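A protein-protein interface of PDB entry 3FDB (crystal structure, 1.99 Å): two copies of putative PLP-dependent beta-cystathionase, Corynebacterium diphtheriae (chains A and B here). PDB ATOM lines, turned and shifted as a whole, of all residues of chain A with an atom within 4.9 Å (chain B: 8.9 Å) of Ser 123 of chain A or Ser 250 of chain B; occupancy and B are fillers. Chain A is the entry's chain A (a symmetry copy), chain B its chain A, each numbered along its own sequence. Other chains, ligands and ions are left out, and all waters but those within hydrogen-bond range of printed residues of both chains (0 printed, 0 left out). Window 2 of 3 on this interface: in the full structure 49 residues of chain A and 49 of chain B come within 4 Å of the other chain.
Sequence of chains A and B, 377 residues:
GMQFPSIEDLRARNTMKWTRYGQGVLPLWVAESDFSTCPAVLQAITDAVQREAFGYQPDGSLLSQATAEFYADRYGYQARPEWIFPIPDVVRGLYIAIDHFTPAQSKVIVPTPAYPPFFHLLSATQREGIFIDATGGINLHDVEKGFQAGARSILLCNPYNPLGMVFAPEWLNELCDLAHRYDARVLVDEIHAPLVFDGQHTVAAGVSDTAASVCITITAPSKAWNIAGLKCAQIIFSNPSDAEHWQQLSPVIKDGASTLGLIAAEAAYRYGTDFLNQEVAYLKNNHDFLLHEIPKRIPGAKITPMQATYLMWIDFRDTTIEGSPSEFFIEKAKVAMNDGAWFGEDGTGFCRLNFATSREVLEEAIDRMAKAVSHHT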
ATOM      1  N   PHE A 119      23.317  -1.578   5.311  1.00  0.00           N
ATOM      2  CA  PHE A 119      22.849  -0.453   4.495  1.00  0.00           C
ATOM      3  C   PHE A 119      22.338   0.661   5.436  1.00  0.00           C
ATOM      4  O   PHE A 119      22.550   1.844   5.172  1.00  0.00           O
ATOM      5  CB  PHE A 119      21.801  -0.901   3.471  1.00  0.00           C
ATOM      6  CG  PHE A 119      22.329  -1.918   2.474  1.00  0.00           C
ATOM      7  CD1 PHE A 119      23.080  -1.529   1.392  1.00  0.00           C
ATOM      8  CD2 PHE A 119      22.111  -3.268   2.660  1.00  0.00           C
ATOM      9  CE1 PHE A 119      23.594  -2.478   0.501  1.00  0.00           C
ATOM     10  CE2 PHE A 119      22.611  -4.197   1.773  1.00  0.00           C
ATOM     11  CZ  PHE A 119      23.354  -3.800   0.700  1.00  0.00           C
ATOM     12  N   HIS A 120      21.719   0.274   6.552  1.00  0.00           N
ATOM     13  CA  HIS A 120      21.322   1.262   7.566  1.00  0.00           C
ATOM     14  C   HIS A 120      22.508   1.845   8.303  1.00  0.00           C
ATOM     15  O   HIS A 120      22.447   2.985   8.768  1.00  0.00           O
ATOM     16  CB  HIS A 120      20.356   0.661   8.560  1.00  0.00           C
ATOM     17  CG  HIS A 120      19.092   0.204   7.935  1.00  0.00           C
ATOM     18  ND1 HIS A 120      18.505  -1.005   8.239  1.00  0.00           N
ATOM     19  CD2 HIS A 120      18.298   0.795   7.005  1.00  0.00           C
ATOM     20  CE1 HIS A 120      17.397  -1.133   7.524  1.00  0.00           C
ATOM     21  NE2 HIS A 120      17.251  -0.058   6.767  1.00  0.00           N
ATOM     22  N   LEU A 121      23.593   1.079   8.400  1.00  0.00           N
ATOM     23  CA  LEU A 121      24.785   1.568   9.030  1.00  0.00           C
ATOM     24  C   LEU A 121      25.365   2.674   8.180  1.00  0.00           C
ATOM     25  O   LEU A 121      25.820   3.695   8.706  1.00  0.00           O
ATOM     26  CB  LEU A 121      25.770   0.433   9.197  1.00  0.00           C
ATOM     27  CG  LEU A 121      27.021   0.551  10.018  1.00  0.00           C
ATOM     28  CD1 LEU A 121      26.772   1.036  11.485  1.00  0.00           C
ATOM     29  CD2 LEU A 121      27.654  -0.863   9.955  1.00  0.00           C
ATOM     30  N   LEU A 122      25.362   2.487   6.867  1.00  0.00           N
ATOM     31  CA  LEU A 122      25.857   3.536   5.940  1.00  0.00           C
ATOM     32  C   LEU A 122      25.024   4.848   6.000  1.00  0.00           C
ATOM     33  O   LEU A 122      25.553   5.959   5.897  1.00  0.00           O
ATOM     34  CB  LEU A 122      25.867   3.008   4.482  1.00  0.00           C
ATOM     35  CG  LEU A 122      26.940   1.949   4.076  1.00  0.00           C
ATOM     36  CD1 LEU A 122      26.750   1.465   2.610  1.00  0.00           C
ATOM     37  CD2 LEU A 122      28.351   2.514   4.279  1.00  0.00           C
ATOM     38  N   SER A 123      23.711   4.709   6.124  1.00  0.00           N
ATOM     39  CA  SER A 123      22.856   5.886   6.188  1.00  0.00           C
ATOM     40  C   SER A 123      23.038   6.575   7.535  1.00  0.00           C
ATOM     41  O   SER A 123      23.122   7.801   7.585  1.00  0.00           O
ATOM     42  CB  SER A 123      21.383   5.533   5.922  1.00  0.00           C
ATOM     43  OG  SER A 123      20.914   4.587   6.863  1.00  0.00           O
ATOM     44  N   ALA A 124      23.160   5.798   8.609  1.00  0.00           N
ATOM     45  CA  ALA A 124      23.376   6.369   9.947  1.00  0.00           C
ATOM     46  C   ALA A 124      24.701   7.115  10.029  1.00  0.00           C
ATOM     47  O   ALA A 124      24.756   8.196  10.602  1.00  0.00           O
ATOM     48  CB  ALA A 124      23.306   5.295  11.041  1.00  0.00           C
ATOM     49  N   THR A 125      25.765   6.563   9.452  1.00  0.00           N
ATOM     50  CA  THR A 125      27.090   7.222   9.485  1.00  0.00           C
ATOM     51  C   THR A 125      27.269   8.273   8.383  1.00  0.00           C
ATOM     52  O   THR A 125      28.272   8.978   8.336  1.00  0.00           O
ATOM     53  CB  THR A 125      28.201   6.184   9.362  1.00  0.00           C
ATOM     54  OG1 THR A 125      28.064   5.455   8.130  1.00  0.00           O
ATOM     55  CG2 THR A 125      28.125   5.207  10.522  1.00  0.00           C
ATOM     56  N   GLN A 126      26.309   8.339   7.470  1.00  0.00           N
ATOM     57  CA  GLN A 126      26.363   9.233   6.313  1.00  0.00           C
ATOM     58  C   GLN A 126      27.574   9.007   5.422  1.00  0.00           C
ATOM     59  O   GLN A 126      28.190   9.946   4.921  1.00  0.00           O
ATOM     60  CB  GLN A 126      26.230  10.683   6.772  1.00  0.00           C
ATOM     61  CG  GLN A 126      24.964  10.863   7.628  1.00  0.00           C
ATOM     62  CD  GLN A 126      24.851  12.238   8.261  1.00  0.00           C
ATOM     63  OE1 GLN A 126      24.960  13.249   7.579  1.00  0.00           O
ATOM     64  NE2 GLN A 126      24.608  12.277   9.573  1.00  0.00           N
ATOM     65  N   ILE B  96      19.850  11.851  20.753  1.00  0.00           N
ATOM     66  CA  ILE B  96      19.232  11.867  19.419  1.00  0.00           C
ATOM     67  C   ILE B  96      18.481  13.181  19.208  1.00  0.00           C
ATOM     68  O   ILE B  96      18.585  13.822  18.148  1.00  0.00           O
ATOM     69  CB  ILE B  96      18.263  10.671  19.212  1.00  0.00           C
ATOM     70  CG1 ILE B  96      19.024   9.327  19.357  1.00  0.00           C
ATOM     71  CG2 ILE B  96      17.560  10.796  17.844  1.00  0.00           C
ATOM     72  CD1 ILE B  96      18.081   8.105  19.641  1.00  0.00           C
ATOM     73  N   HIS B 100      19.653  15.475  16.197  1.00  0.00           N
ATOM     74  CA  HIS B 100      18.767  15.459  15.038  1.00  0.00           C
ATOM     75  C   HIS B 100      17.621  16.444  15.032  1.00  0.00           C
ATOM     76  O   HIS B 100      17.069  16.661  13.976  1.00  0.00           O
ATOM     77  CB  HIS B 100      18.238  14.036  14.793  1.00  0.00           C
ATOM     78  CG  HIS B 100      19.312  13.095  14.370  1.00  0.00           C
ATOM     79  ND1 HIS B 100      19.791  13.049  13.078  1.00  0.00           N
ATOM     80  CD2 HIS B 100      20.070  12.241  15.086  1.00  0.00           C
ATOM     81  CE1 HIS B 100      20.778  12.175  13.018  1.00  0.00           C
ATOM     82  NE2 HIS B 100      20.968  11.675  14.225  1.00  0.00           N
ATOM     83  N   HIS B 245       9.788  12.888  11.342  1.00  0.00           N
ATOM     84  CA  HIS B 245      11.246  13.055  11.285  1.00  0.00           C
ATOM     85  C   HIS B 245      11.930  11.867  11.991  1.00  0.00           C
ATOM     86  O   HIS B 245      12.880  11.288  11.478  1.00  0.00           O
ATOM     87  CB  HIS B 245      11.641  14.401  11.902  1.00  0.00           C
ATOM     88  CG  HIS B 245      13.084  14.732  11.727  1.00  0.00           C
ATOM     89  ND1 HIS B 245      13.930  14.941  12.785  1.00  0.00           N
ATOM     90  CD2 HIS B 245      13.842  14.845  10.614  1.00  0.00           C
ATOM     91  CE1 HIS B 245      15.150  15.159  12.336  1.00  0.00           C
ATOM     92  NE2 HIS B 245      15.125  15.113  11.024  1.00  0.00           N
ATOM     93  N   TRP B 246      11.397  11.464  13.131  1.00  0.00           N
ATOM     94  CA  TRP B 246      11.868  10.282  13.836  1.00  0.00           C
ATOM     95  C   TRP B 246      11.790   9.022  12.974  1.00  0.00           C
ATOM     96  O   TRP B 246      12.759   8.241  12.865  1.00  0.00           O
ATOM     97  CB  TRP B 246      11.034  10.094  15.088  1.00  0.00           C
ATOM     98  CG  TRP B 246      11.384   8.904  15.862  1.00  0.00           C
ATOM     99  CD1 TRP B 246      10.787   7.684  15.793  1.00  0.00           C
ATOM    100  CD2 TRP B 246      12.438   8.787  16.820  1.00  0.00           C
ATOM    101  NE1 TRP B 246      11.387   6.817  16.680  1.00  0.00           N
ATOM    102  CE2 TRP B 246      12.394   7.473  17.329  1.00  0.00           C
ATOM    103  CE3 TRP B 246      13.400   9.673  17.319  1.00  0.00           C
ATOM    104  CZ2 TRP B 246      13.275   7.025  18.293  1.00  0.00           C
ATOM    105  CZ3 TRP B 246      14.264   9.231  18.285  1.00  0.00           C
ATOM    106  CH2 TRP B 246      14.205   7.920  18.760  1.00  0.00           C
ATOM    107  N   GLN B 247      10.639   8.826  12.342  1.00  0.00           N
ATOM    108  CA  GLN B 247      10.441   7.655  11.507  1.00  0.00           C
ATOM    109  C   GLN B 247      11.400   7.623  10.325  1.00  0.00           C
ATOM    110  O   GLN B 247      11.796   6.551   9.889  1.00  0.00           O
ATOM    111  CB  GLN B 247       8.960   7.520  11.093  1.00  0.00           C
ATOM    112  CG  GLN B 247       8.148   7.025  12.296  1.00  0.00           C
ATOM    113  CD  GLN B 247       6.662   6.822  12.055  1.00  0.00           C
ATOM    114  OE1 GLN B 247       5.926   7.764  11.739  1.00  0.00           O
ATOM    115  NE2 GLN B 247       6.201   5.587  12.277  1.00  0.00           N
ATOM    116  N   GLN B 248      11.822   8.784   9.843  1.00  0.00           N
ATOM    117  CA  GLN B 248      12.783   8.855   8.724  1.00  0.00           C
ATOM    118  C   GLN B 248      14.241   8.574   9.117  1.00  0.00           C
ATOM    119  O   GLN B 248      15.090   8.404   8.244  1.00  0.00           O
ATOM    120  CB  GLN B 248      12.710  10.221   8.023  1.00  0.00           C
ATOM    121  CG  GLN B 248      11.405  10.466   7.268  1.00  0.00           C
ATOM    122  CD  GLN B 248      11.158  11.955   6.987  1.00  0.00           C
ATOM    123  OE1 GLN B 248      11.870  12.826   7.522  1.00  0.00           O
ATOM    124  NE2 GLN B 248      10.141  12.253   6.158  1.00  0.00           N
ATOM    125  N   LEU B 249      14.545   8.560  10.409  1.00  0.00           N
ATOM    126  CA  LEU B 249      15.895   8.273  10.860  1.00  0.00           C
ATOM    127  C   LEU B 249      16.251   6.820  10.594  1.00  0.00           C
ATOM    128  O   LEU B 249      15.378   5.954  10.666  1.00  0.00           O
ATOM    129  CB  LEU B 249      16.025   8.511  12.377  1.00  0.00           C
ATOM    130  CG  LEU B 249      15.835   9.960  12.838  1.00  0.00           C
ATOM    131  CD1 LEU B 249      15.808  10.024  14.340  1.00  0.00           C
ATOM    132  CD2 LEU B 249      16.955  10.869  12.234  1.00  0.00           C
ATOM    133  N   SER B 250      17.520   6.568  10.270  1.00  0.00           N
ATOM    134  CA  SER B 250      18.005   5.207  10.153  1.00  0.00           C
ATOM    135  C   SER B 250      17.682   4.406  11.423  1.00  0.00           C
ATOM    136  O   SER B 250      17.823   4.893  12.559  1.00  0.00           O
ATOM    137  CB  SER B 250      19.519   5.175   9.945  1.00  0.00           C
ATOM    138  OG  SER B 250      20.016   3.844  10.045  1.00  0.00           O
ATOM    139  N   PRO B 251      17.238   3.167  11.248  1.00  0.00           N
ATOM    140  CA  PRO B 251      17.010   2.304  12.422  1.00  0.00           C
ATOM    141  C   PRO B 251      18.212   2.191  13.338  1.00  0.00           C
ATOM    142  O   PRO B 251      18.067   2.055  14.555  1.00  0.00           O
ATOM    143  CB  PRO B 251      16.685   0.938  11.797  1.00  0.00           C
ATOM    144  CG  PRO B 251      16.304   1.200  10.419  1.00  0.00           C
ATOM    145  CD  PRO B 251      16.878   2.515   9.983  1.00  0.00           C
ATOM    146  N   VAL B 252      19.426   2.230  12.785  1.00  0.00           N
ATOM    147  CA  VAL B 252      20.630   2.131  13.594  1.00  0.00           C
ATOM    148  C   VAL B 252      20.684   3.281  14.602  1.00  0.00           C
ATOM    149  O   VAL B 252      21.215   3.123  15.698  1.00  0.00           O
ATOM    150  CB  VAL B 252      21.924   2.124  12.703  1.00  0.00           C
ATOM    151  CG1 VAL B 252      23.204   2.228  13.553  1.00  0.00           C
ATOM    152  CG2 VAL B 252      21.942   0.861  11.824  1.00  0.00           C
ATOM    153  N   ILE B 253      20.114   4.433  14.262  1.00  0.00           N
ATOM    154  CA  ILE B 253      20.155   5.568  15.199  1.00  0.00           C
ATOM    155  C   ILE B 253      19.235   5.325  16.407  1.00  0.00           C
ATOM    156  O   ILE B 253      19.548   5.738  17.517  1.00  0.00           O
ATOM    157  CB  ILE B 253      19.796   6.925  14.480  1.00  0.00           C
ATOM    158  CG1 ILE B 253      20.902   7.279  13.475  1.00  0.00           C
ATOM    159  CG2 ILE B 253      19.574   8.050  15.518  1.00  0.00           C
ATOM    160  CD1 ILE B 253      20.537   8.350  12.421  1.00  0.00           C
ATOM    161  N   LYS B 254      18.123   4.634  16.165  1.00  0.00           N
ATOM    162  CA  LYS B 254      17.040   4.470  17.132  1.00  0.00           C
ATOM    163  C   LYS B 254      17.026   3.165  17.948  1.00  0.00           C
ATOM    164  O   LYS B 254      16.254   3.048  18.914  1.00  0.00           O
ATOM    165  CB  LYS B 254      15.703   4.562  16.365  1.00  0.00           C
ATOM    166  CG  LYS B 254      15.464   5.886  15.692  1.00  0.00           C
ATOM    167  CD  LYS B 254      14.176   5.914  14.834  1.00  0.00           C
ATOM    168  CE  LYS B 254      14.287   5.060  13.585  1.00  0.00           C
ATOM    169  NZ  LYS B 254      13.286   5.397  12.563  1.00  0.00           N
ATOM    170  N   ASP B 255      17.834   2.185  17.580  1.00  0.00           N
ATOM    171  CA  ASP B 255      17.702   0.901  18.223  1.00  0.00           C
ATOM    172  C   ASP B 255      18.537   0.829  19.500  1.00  0.00           C
ATOM    173  O   ASP B 255      19.346   1.717  19.774  1.00  0.00           O
ATOM    174  CB  ASP B 255      18.026  -0.223  17.235  1.00  0.00           C
ATOM    175  CG  ASP B 255      16.999  -0.336  16.089  1.00  0.00           C
ATOM    176  OD1 ASP B 255      15.975   0.406  16.040  1.00  0.00           O
ATOM    177  OD2 ASP B 255      17.253  -1.150  15.192  1.00  0.00           O
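OG of Ser 250 of chain B is in hydrogen-bond range of O of His 120 of chain A (2.9 Å). The side-chain hydroxyl of Ser 123 of chain A lies within hydrogen-bond range of the side-chain hydroxyl of Ser 250 of chain B, 3.4 Å away.
The side-chain hydroxyl of Ser 250 of chain B lies close to the backbone NH of Val 252 of chain B (3.2 Å). O of His 120 of chain A lies within hydrogen-bond range of OG of Ser 123 of chain A (2.9 Å). The backbone carbonyl oxygen (O) of Leu 121 of chain A lies within hydrogen-bond range of the side-chain hydroxyl (OG1) of Thr 125 of chain A (2.9 Å).
CD2 of His 120 of chain A touches CD of Pro 251 of chain B (3.7 Å). His 120 of chain A touches Val 252 of chain B (CB to CG2, 3.6 Å). CG2 of Val 252 of chain B touches N of Leu 121 of chain A (3.8 Å). Ala 124 of chain A touches Ser 250 of chain B. Ala 124 of chain A touches Val 252 of chain B. Ile 253 of chain B touches Ala 124 of chain A (CG1 to CB, 3.95 Å).
Of the printed residues of chain B, His 120 of chain A touches Ser 250, Pro 251 and Val 252. Of the printed residues of chain B, Leu 121 of chain A touches Val 252. Ser 123 of chain A touches one residue of chain B. Of chain B, only Ser 250 (3.7 Å), Val 252 (3.8 Å) and Ile 253 (3.95 Å) come within 4 Å of Ala 124 of chain A. Printed residues of chain A within 4 Å of Ser 250 of chain B: His 120 (2.9 Å), Ser 123 (3.4 Å) and Ala 124 (3.7 Å). Of the printed residues of chain A, Pro 251 of chain B touches His 120. Of the printed residues of chain A, Val 252 of chain B touches His 120 (3.6 Å), Leu 121 (3.8 Å) and Ala 124 (3.8 Å). Lys 254 of chain B touches none of the printed residues of chain A. The nearest printed residue of chain B that does not touch Ser 123 of chain A is Pro 251 of chain B (5.5 Å). The nearest residue of chain A that does not touch Ser 250 of chain B is Leu 121 of chain A (4.8 Å).
Of the 13 printed residues of chain B, 4 touch a printed residue of chain A. Printed residues of chain B that touch a printed residue of chain A: Ser 250, Pro 251, Val 252 and Ile 253. Hydrophobic or aromatic side chains of chain B within 4 Å of the printed part of chain A: Pro 251, Val 252 and Ile 253. Of the 8 printed residues of chain A, 4 touch a printed residue of chain B. Hydrophobic or aromatic side chains of chain A within 4 Å of the printed part of chain B: His 120 and Ala 124. Along chain A the printed residues that touch a printed residue of chain B span positions 120 to 124. Among the printed residues, no Asp or Glu carboxylate lies within 4 Å of a Lys or Arg side-chain nitrogen of the other chain.
No position is printed for both chains.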
